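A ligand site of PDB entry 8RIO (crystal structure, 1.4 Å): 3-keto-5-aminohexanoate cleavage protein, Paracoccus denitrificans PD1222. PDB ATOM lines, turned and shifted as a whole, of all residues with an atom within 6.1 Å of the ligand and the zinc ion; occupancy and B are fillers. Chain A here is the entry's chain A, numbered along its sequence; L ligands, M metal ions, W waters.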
ATOM      1  N   ALA A  12      14.816 -19.895 -15.758  1.00  0.00           N
ATOM      2  CA  ALA A  12      14.333 -19.203 -14.546  1.00  0.00           C
ATOM      3  C   ALA A  12      13.293 -18.173 -14.996  1.00  0.00           C
ATOM      4  O   ALA A  12      13.647 -17.146 -15.584  1.00  0.00           O
ATOM      5  CB  ALA A  12      15.513 -18.560 -13.772  1.00  0.00           C
ATOM      6  N   GLY A  15      11.507 -15.048 -11.078  1.00  0.00           N
ATOM      7  CA  GLY A  15      12.444 -14.517 -10.052  1.00  0.00           C
ATOM      8  C   GLY A  15      11.806 -13.509  -9.105  1.00  0.00           C
ATOM      9  O   GLY A  15      10.573 -13.435  -8.945  1.00  0.00           O
ATOM     10  N   ALA A  16      12.701 -12.731  -8.481  1.00  0.00           N
ATOM     11  CA  ALA A  16      12.347 -11.702  -7.523  1.00  0.00           C
ATOM     12  C   ALA A  16      13.208 -10.459  -7.705  1.00  0.00           C
ATOM     13  O   ALA A  16      12.989  -9.487  -6.982  1.00  0.00           O
ATOM     14  CB  ALA A  16      12.496 -12.254  -6.070  1.00  0.00           C
ATOM     15  N   ILE A  17      14.153 -10.457  -8.636  1.00  0.00           N
ATOM     16  CA  ILE A  17      15.035  -9.295  -8.840  1.00  0.00           C
ATOM     17  C   ILE A  17      14.412  -8.278  -9.800  1.00  0.00           C
ATOM     18  O   ILE A  17      14.418  -7.083  -9.523  1.00  0.00           O
ATOM     19  CB  ILE A  17      16.411  -9.779  -9.324  1.00  0.00           C
ATOM     20  CG1 ILE A  17      17.189 -10.311  -8.077  1.00  0.00           C
ATOM     21  CG2 ILE A  17      17.179  -8.608 -10.049  1.00  0.00           C
ATOM     22  CD1 ILE A  17      18.475 -11.072  -8.447  1.00  0.00           C
ATOM     23  N   HIS A  49      13.367 -23.125 -12.942  1.00  0.00           N
ATOM     24  CA  HIS A  49      13.601 -22.469 -11.630  1.00  0.00           C
ATOM     25  C   HIS A  49      12.471 -21.489 -11.352  1.00  0.00           C
ATOM     26  O   HIS A  49      12.231 -20.563 -12.145  1.00  0.00           O
ATOM     27  CB  HIS A  49      14.975 -21.783 -11.711  1.00  0.00           C
ATOM     28  CG  HIS A  49      15.350 -20.930 -10.538  1.00  0.00           C
ATOM     29  ND1 HIS A  49      16.452 -21.222  -9.752  1.00  0.00           N
ATOM     30  CD2 HIS A  49      14.966 -19.672 -10.174  1.00  0.00           C
ATOM     31  CE1 HIS A  49      16.612 -20.270  -8.848  1.00  0.00           C
ATOM     32  NE2 HIS A  49      15.716 -19.317  -9.086  1.00  0.00           N
ATOM     33  N   LEU A  50      11.736 -21.704 -10.240  1.00  0.00           N
ATOM     34  CA  LEU A  50      10.456 -21.083  -9.982  1.00  0.00           C
ATOM     35  C   LEU A  50      10.475 -20.202  -8.749  1.00  0.00           C
ATOM     36  O   LEU A  50      10.999 -20.591  -7.697  1.00  0.00           O
ATOM     37  CB  LEU A  50       9.441 -22.208  -9.745  1.00  0.00           C
ATOM     38  CG  LEU A  50       9.071 -22.943 -11.052  1.00  0.00           C
ATOM     39  CD1 LEU A  50       8.302 -24.265 -10.676  1.00  0.00           C
ATOM     40  CD2 LEU A  50       8.211 -22.094 -11.957  1.00  0.00           C
ATOM     41  N   HIS A  51       9.838 -19.032  -8.887  1.00  0.00           N
ATOM     42  CA  HIS A  51       9.382 -18.178  -7.792  1.00  0.00           C
ATOM     43  C   HIS A  51       7.913 -17.896  -8.029  1.00  0.00           C
ATOM     44  O   HIS A  51       7.388 -18.123  -9.127  1.00  0.00           O
ATOM     45  CB  HIS A  51      10.068 -16.806  -7.844  1.00  0.00           C
ATOM     46  CG  HIS A  51      11.564 -16.832  -7.618  1.00  0.00           C
ATOM     47  ND1 HIS A  51      12.163 -16.044  -6.652  1.00  0.00           N
ATOM     48  CD2 HIS A  51      12.584 -17.477  -8.254  1.00  0.00           C
ATOM     49  CE1 HIS A  51      13.476 -16.178  -6.719  1.00  0.00           C
ATOM     50  NE2 HIS A  51      13.748 -17.065  -7.661  1.00  0.00           N
ATOM     51  N   THR A  85      12.853 -21.932  -5.533  1.00  0.00           N
ATOM     52  CA  THR A  85      13.753 -21.017  -4.841  1.00  0.00           C
ATOM     53  C   THR A  85      13.697 -21.176  -3.322  1.00  0.00           C
ATOM     54  O   THR A  85      12.633 -21.473  -2.754  1.00  0.00           O
ATOM     55  CB  THR A  85      13.386 -19.567  -5.211  1.00  0.00           C
ATOM     56  OG1 THR A  85      14.401 -18.690  -4.723  1.00  0.00           O
ATOM     57  CG2 THR A  85      12.037 -19.115  -4.650  1.00  0.00           C
ATOM     58  N   THR A  86      14.831 -20.880  -2.674  1.00  0.00           N
ATOM     59  CA  THR A  86      14.918 -20.642  -1.235  1.00  0.00           C
ATOM     60  C   THR A  86      15.336 -19.234  -0.901  1.00  0.00           C
ATOM     61  O   THR A  86      15.743 -18.972   0.233  1.00  0.00           O
ATOM     62  CB  THR A  86      15.825 -21.661  -0.520  1.00  0.00           C
ATOM     63  OG1 THR A  86      17.194 -21.472  -0.971  1.00  0.00           O
ATOM     64  CG2 THR A  86      15.349 -23.061  -0.756  1.00  0.00           C
ATOM     65  N   GLY A  87      15.194 -18.315  -1.867  1.00  0.00           N
ATOM     66  CA  GLY A  87      15.492 -16.918  -1.580  1.00  0.00           C
ATOM     67  C   GLY A  87      14.348 -16.276  -0.847  1.00  0.00           C
ATOM     68  O   GLY A  87      13.272 -16.832  -0.740  1.00  0.00           O
ATOM     69  N   GLY A  88      14.553 -15.052  -0.443  1.00  0.00           N
ATOM     70  CA  GLY A  88      13.424 -14.330   0.123  1.00  0.00           C
ATOM     71  C   GLY A  88      13.877 -12.953   0.513  1.00  0.00           C
ATOM     72  O   GLY A  88      15.047 -12.597   0.367  1.00  0.00           O
ATOM     73  N   ARG A  97      12.098 -18.960   4.697  1.00  0.00           N
ATOM     74  CA  ARG A  97      12.445 -19.019   3.279  1.00  0.00           C
ATOM     75  C   ARG A  97      12.374 -20.437   2.716  1.00  0.00           C
ATOM     76  O   ARG A  97      12.058 -20.609   1.522  1.00  0.00           O
ATOM     77  CB  ARG A  97      13.888 -18.520   3.090  1.00  0.00           C
ATOM     78  CG  ARG A  97      13.902 -16.969   3.068  1.00  0.00           C
ATOM     79  CD  ARG A  97      15.377 -16.455   3.236  1.00  0.00           C
ATOM     80  NE  ARG A  97      16.196 -17.032   2.188  1.00  0.00           N
ATOM     81  CZ  ARG A  97      17.513 -16.940   2.156  1.00  0.00           C
ATOM     82  NH1 ARG A  97      18.165 -16.178   3.041  1.00  0.00           N
ATOM     83  NH2 ARG A  97      18.171 -17.593   1.214  1.00  0.00           N
ATOM     84  N   SER A 110      16.931 -24.100  -5.054  1.00  0.00           N
ATOM     85  CA  SER A 110      18.110 -23.251  -5.215  1.00  0.00           C
ATOM     86  C   SER A 110      18.736 -22.982  -3.859  1.00  0.00           C
ATOM     87  O   SER A 110      18.074 -23.093  -2.830  1.00  0.00           O
ATOM     88  CB  SER A 110      17.674 -21.938  -5.889  1.00  0.00           C
ATOM     89  OG  SER A 110      17.005 -21.115  -4.947  1.00  0.00           O
ATOM     90  N   ASN A 112      21.624 -20.204  -2.337  1.00  0.00           N
ATOM     91  CA  ASN A 112      22.664 -19.205  -2.452  1.00  0.00           C
ATOM     92  C   ASN A 112      23.744 -19.499  -1.407  1.00  0.00           C
ATOM     93  O   ASN A 112      23.455 -19.657  -0.221  1.00  0.00           O
ATOM     94  CB  ASN A 112      22.053 -17.822  -2.239  1.00  0.00           C
ATOM     95  CG  ASN A 112      23.044 -16.681  -2.491  1.00  0.00           C
ATOM     96  OD1 ASN A 112      24.280 -16.858  -2.472  1.00  0.00           O
ATOM     97  ND2 ASN A 112      22.512 -15.491  -2.694  1.00  0.00           N
ATOM     98  N   PHE A 147      21.570 -10.204   0.647  1.00  0.00           N
ATOM     99  CA  PHE A 147      21.054 -11.578   0.614  1.00  0.00           C
ATOM    100  C   PHE A 147      21.806 -12.294   1.723  1.00  0.00           C
ATOM    101  O   PHE A 147      23.032 -12.440   1.636  1.00  0.00           O
ATOM    102  CB  PHE A 147      21.342 -12.262  -0.719  1.00  0.00           C
ATOM    103  CG  PHE A 147      20.759 -11.560  -1.976  1.00  0.00           C
ATOM    104  CD1 PHE A 147      19.614 -10.778  -1.891  1.00  0.00           C
ATOM    105  CD2 PHE A 147      21.348 -11.733  -3.206  1.00  0.00           C
ATOM    106  CE1 PHE A 147      19.068 -10.153  -3.060  1.00  0.00           C
ATOM    107  CE2 PHE A 147      20.807 -11.090  -4.391  1.00  0.00           C
ATOM    108  CZ  PHE A 147      19.671 -10.332  -4.275  1.00  0.00           C
ATOM    109  N   ASN A 149      22.988 -15.429   3.821  1.00  0.00           N
ATOM    110  CA  ASN A 149      23.100 -16.880   3.755  1.00  0.00           C
ATOM    111  C   ASN A 149      24.350 -17.250   4.535  1.00  0.00           C
ATOM    112  O   ASN A 149      25.409 -17.558   3.968  1.00  0.00           O
ATOM    113  CB  ASN A 149      23.216 -17.380   2.314  1.00  0.00           C
ATOM    114  CG  ASN A 149      22.022 -16.984   1.492  1.00  0.00           C
ATOM    115  OD1 ASN A 149      20.943 -17.560   1.645  1.00  0.00           O
ATOM    116  ND2 ASN A 149      22.158 -15.922   0.711  1.00  0.00           N
ATOM    117  N   GLU A 171      23.908 -21.836  -6.044  1.00  0.00           N
ATOM    118  CA  GLU A 171      24.178 -20.590  -6.743  1.00  0.00           C
ATOM    119  C   GLU A 171      25.396 -19.905  -6.129  1.00  0.00           C
ATOM    120  O   GLU A 171      25.382 -19.558  -4.960  1.00  0.00           O
ATOM    121  CB  GLU A 171      22.945 -19.683  -6.656  1.00  0.00           C
ATOM    122  CG  GLU A 171      21.689 -20.236  -7.378  1.00  0.00           C
ATOM    123  CD  GLU A 171      20.548 -19.276  -7.310  1.00  0.00           C
ATOM    124  OE1 GLU A 171      20.538 -18.397  -6.407  1.00  0.00           O
ATOM    125  OE2 GLU A 171      19.612 -19.474  -8.065  1.00  0.00           O
ATOM    126  N   TYR A 173      28.002 -16.841  -6.544  1.00  0.00           N
ATOM    127  CA  TYR A 173      28.050 -15.503  -7.155  1.00  0.00           C
ATOM    128  C   TYR A 173      29.443 -14.934  -7.150  1.00  0.00           C
ATOM    129  O   TYR A 173      29.639 -13.826  -7.658  1.00  0.00           O
ATOM    130  CB  TYR A 173      27.075 -14.555  -6.393  1.00  0.00           C
ATOM    131  CG  TYR A 173      25.620 -14.905  -6.490  1.00  0.00           C
ATOM    132  CD1 TYR A 173      25.071 -15.917  -5.735  1.00  0.00           C
ATOM    133  CD2 TYR A 173      24.803 -14.235  -7.376  1.00  0.00           C
ATOM    134  CE1 TYR A 173      23.722 -16.292  -5.867  1.00  0.00           C
ATOM    135  CE2 TYR A 173      23.440 -14.575  -7.492  1.00  0.00           C
ATOM    136  CZ  TYR A 173      22.941 -15.595  -6.731  1.00  0.00           C
ATOM    137  OH  TYR A 173      21.580 -15.993  -6.879  1.00  0.00           O
ATOM    138  N   LEU A 202      25.951  -9.639 -11.654  1.00  0.00           N
ATOM    139  CA  LEU A 202      25.059  -8.910 -10.781  1.00  0.00           C
ATOM    140  C   LEU A 202      25.860  -7.932  -9.937  1.00  0.00           C
ATOM    141  O   LEU A 202      27.002  -8.196  -9.556  1.00  0.00           O
ATOM    142  CB  LEU A 202      24.305  -9.865  -9.841  1.00  0.00           C
ATOM    143  CG  LEU A 202      23.291 -10.745 -10.564  1.00  0.00           C
ATOM    144  CD1 LEU A 202      22.534 -11.682  -9.536  1.00  0.00           C
ATOM    145  CD2 LEU A 202      22.245  -9.911 -11.227  1.00  0.00           C
ATOM    146  N   ARG A 254      21.917 -21.594 -18.096  1.00  0.00           N
ATOM    147  CA  ARG A 254      20.690 -21.058 -17.524  1.00  0.00           C
ATOM    148  C   ARG A 254      20.300 -19.801 -18.291  1.00  0.00           C
ATOM    149  O   ARG A 254      21.129 -18.895 -18.465  1.00  0.00           O
ATOM    150  CB  ARG A 254      20.865 -20.771 -16.025  1.00  0.00           C
ATOM    151  CG  ARG A 254      19.664 -20.098 -15.367  1.00  0.00           C
ATOM    152  CD  ARG A 254      19.826 -20.127 -13.850  1.00  0.00           C
ATOM    153  NE  ARG A 254      18.915 -19.078 -13.330  1.00  0.00           N
ATOM    154  CZ  ARG A 254      18.705 -18.904 -12.024  1.00  0.00           C
ATOM    155  NH1 ARG A 254      19.149 -19.803 -11.142  1.00  0.00           N
ATOM    156  NH2 ARG A 254      18.103 -17.759 -11.608  1.00  0.00           N
ATOM    157  N   GLU A 258      13.796 -14.186 -15.359  1.00  0.00           N
ATOM    158  CA  GLU A 258      14.275 -13.869 -14.000  1.00  0.00           C
ATOM    159  C   GLU A 258      15.636 -13.187 -14.077  1.00  0.00           C
ATOM    160  O   GLU A 258      15.954 -12.324 -13.264  1.00  0.00           O
ATOM    161  CB  GLU A 258      14.413 -15.180 -13.205  1.00  0.00           C
ATOM    162  CG  GLU A 258      15.274 -15.008 -11.952  1.00  0.00           C
ATOM    163  CD  GLU A 258      15.072 -16.098 -10.928  1.00  0.00           C
ATOM    164  OE1 GLU A 258      14.194 -16.945 -11.082  1.00  0.00           O
ATOM    165  OE2 GLU A 258      15.844 -16.105  -9.913  1.00  0.00           O
ATOM    166  N   ASP A 259      16.437 -13.597 -15.075  1.00  0.00           N
ATOM    167  CA  ASP A 259      17.857 -13.267 -15.141  1.00  0.00           C
ATOM    168  C   ASP A 259      18.183 -12.176 -16.165  1.00  0.00           C
ATOM    169  O   ASP A 259      19.153 -11.432 -15.975  1.00  0.00           O
ATOM    170  CB  ASP A 259      18.647 -14.540 -15.565  1.00  0.00           C
ATOM    171  CG  ASP A 259      18.479 -15.701 -14.610  1.00  0.00           C
ATOM    172  OD1 ASP A 259      18.276 -15.444 -13.398  1.00  0.00           O
ATOM    173  OD2 ASP A 259      18.648 -16.840 -15.042  1.00  0.00           O
HETATM  174  N1  LIG L   1      18.415 -14.544  -6.313  1.00  0.00           N
HETATM  175  C1  LIG L   1      18.307 -15.877  -5.689  1.00  0.00           C
HETATM  176  C2  LIG L   1      17.052 -16.529  -6.208  1.00  0.00           C
HETATM  177  O1  LIG L   1      16.437 -15.768  -7.015  1.00  0.00           O
HETATM  178  C3  LIG L   1      18.284 -15.544  -4.202  1.00  0.00           C
HETATM  179  C4  LIG L   1      19.224 -14.362  -4.111  1.00  0.00           C
HETATM  180  C5  LIG L   1      19.096 -13.590  -5.430  1.00  0.00           C
HETATM  181  O2  LIG L   1      16.719 -17.751  -5.949  1.00  0.00           O
HETATM  182 ZN    ZN M   1      15.727 -17.363  -8.378  1.00  0.00          ZN
HETATM  183  O   HOH W   1      15.909 -13.183  -6.028  1.00  0.00           O
HETATM  184  O   HOH W   2      15.423 -13.478  -8.623  1.00  0.00           O
HETATM  185  O   HOH W   3      19.843 -15.567  -1.074  1.00  0.00           O
HETATM  186  O   HOH W   4      18.512 -18.818  -4.505  1.00  0.00           O
HETATM  187  O   HOH W   5      18.021 -17.507  -8.757  1.00  0.00           O
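The side-chain carboxylate (OE2) of Glu 258 lies close to the guanidinium group (NH2) of Arg 254 (3.3 Å).
The side-chain carboxylate (OE1) of Glu 258 sits close to the backbone NH (N) of Gly 15.
The backbone carbonyl oxygen (O) of Ala 12 sits at hydrogen-bond distance from the backbone NH (N) of Glu 258, at 3.0 Å.
A ring nitrogen (ND1) of His 49 lies within hydrogen-bond range of the guanidinium group (NH1) of Arg 254.
A ring nitrogen (NE2) of His 51 lies close to the side-chain hydroxyl (OG1) of Thr 85 (3.4 Å).
OG1 of Thr 85 sits at hydrogen-bond distance from N of Gly 87, at 3.0 Å.
The backbone NH (N) of Thr 85 lies within hydrogen-bond range of the backbone carbonyl oxygen (O) of Leu 50 (3.1 Å).
The side-chain carboxylate of Glu 171 is in salt-bridge range of the guanidinium group of Arg 254, 3.1 Å away.
Water W5 lies within hydrogen-bond range of the side-chain carboxylate of Glu 171 (2.6 Å), the guanidinium group of Arg 254 (2.9 Å) and an oxygen (O2) of the ligand (3.1 Å).
Water W4 lies within hydrogen-bond range of O2 of the ligand (2.5 Å), OG of Ser 110 (2.8 Å) and OE1 of Glu 171 (2.8 Å).
OE2 of Glu 258 is bound to the zinc ion (2.0 Å).
NE2 of His 49 binds the zinc ion, at 2.1 Å.
The zinc ion is bound by NE2 of His 51.
The zinc ion is bound by O1 of the ligand (2.2 Å).
Water W5 binds the zinc ion (2.3 Å).
Slightly farther from the zinc ion lies an oxygen (O2) of the ligand (2.7 Å).
An oxygen (O2) of the ligand lies within hydrogen-bond range of the side-chain hydroxyl of Thr 85 (2.8 Å).
Of the 22 residues printed, 3 come within 4 Å of the zinc ion.
The nearest printed residue that does not touch the zinc ion is Arg 254 (4.03 Å).
Ile 17 touches the ligand (CD1 to C5, 3.98 Å).
OG of Ser 110 touches O2 of the ligand, at 3.5 Å.
Asn 112 touches the ligand.
CE2 of Phe 147 touches C5 of the ligand (3.2 Å).
OE1 of Glu 171 touches C1 of the ligand, at 3.4 Å.
Tyr 173 touches the ligand (OH to C1, 3.5 Å).
Hydrophobic or aromatic side chains that line the ligand: Ile 17, His 49, His 51 and Phe 147.
Ten residues have an atom within 4 Å of the ligand: Ile 17, His 49, His 51, Thr 85, Ser 110, Asn 112, Phe 147, Glu 171, Tyr 173 and Glu 258.
The nearest printed residue that does not touch the ligand is Gly 87 (4.1 Å).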
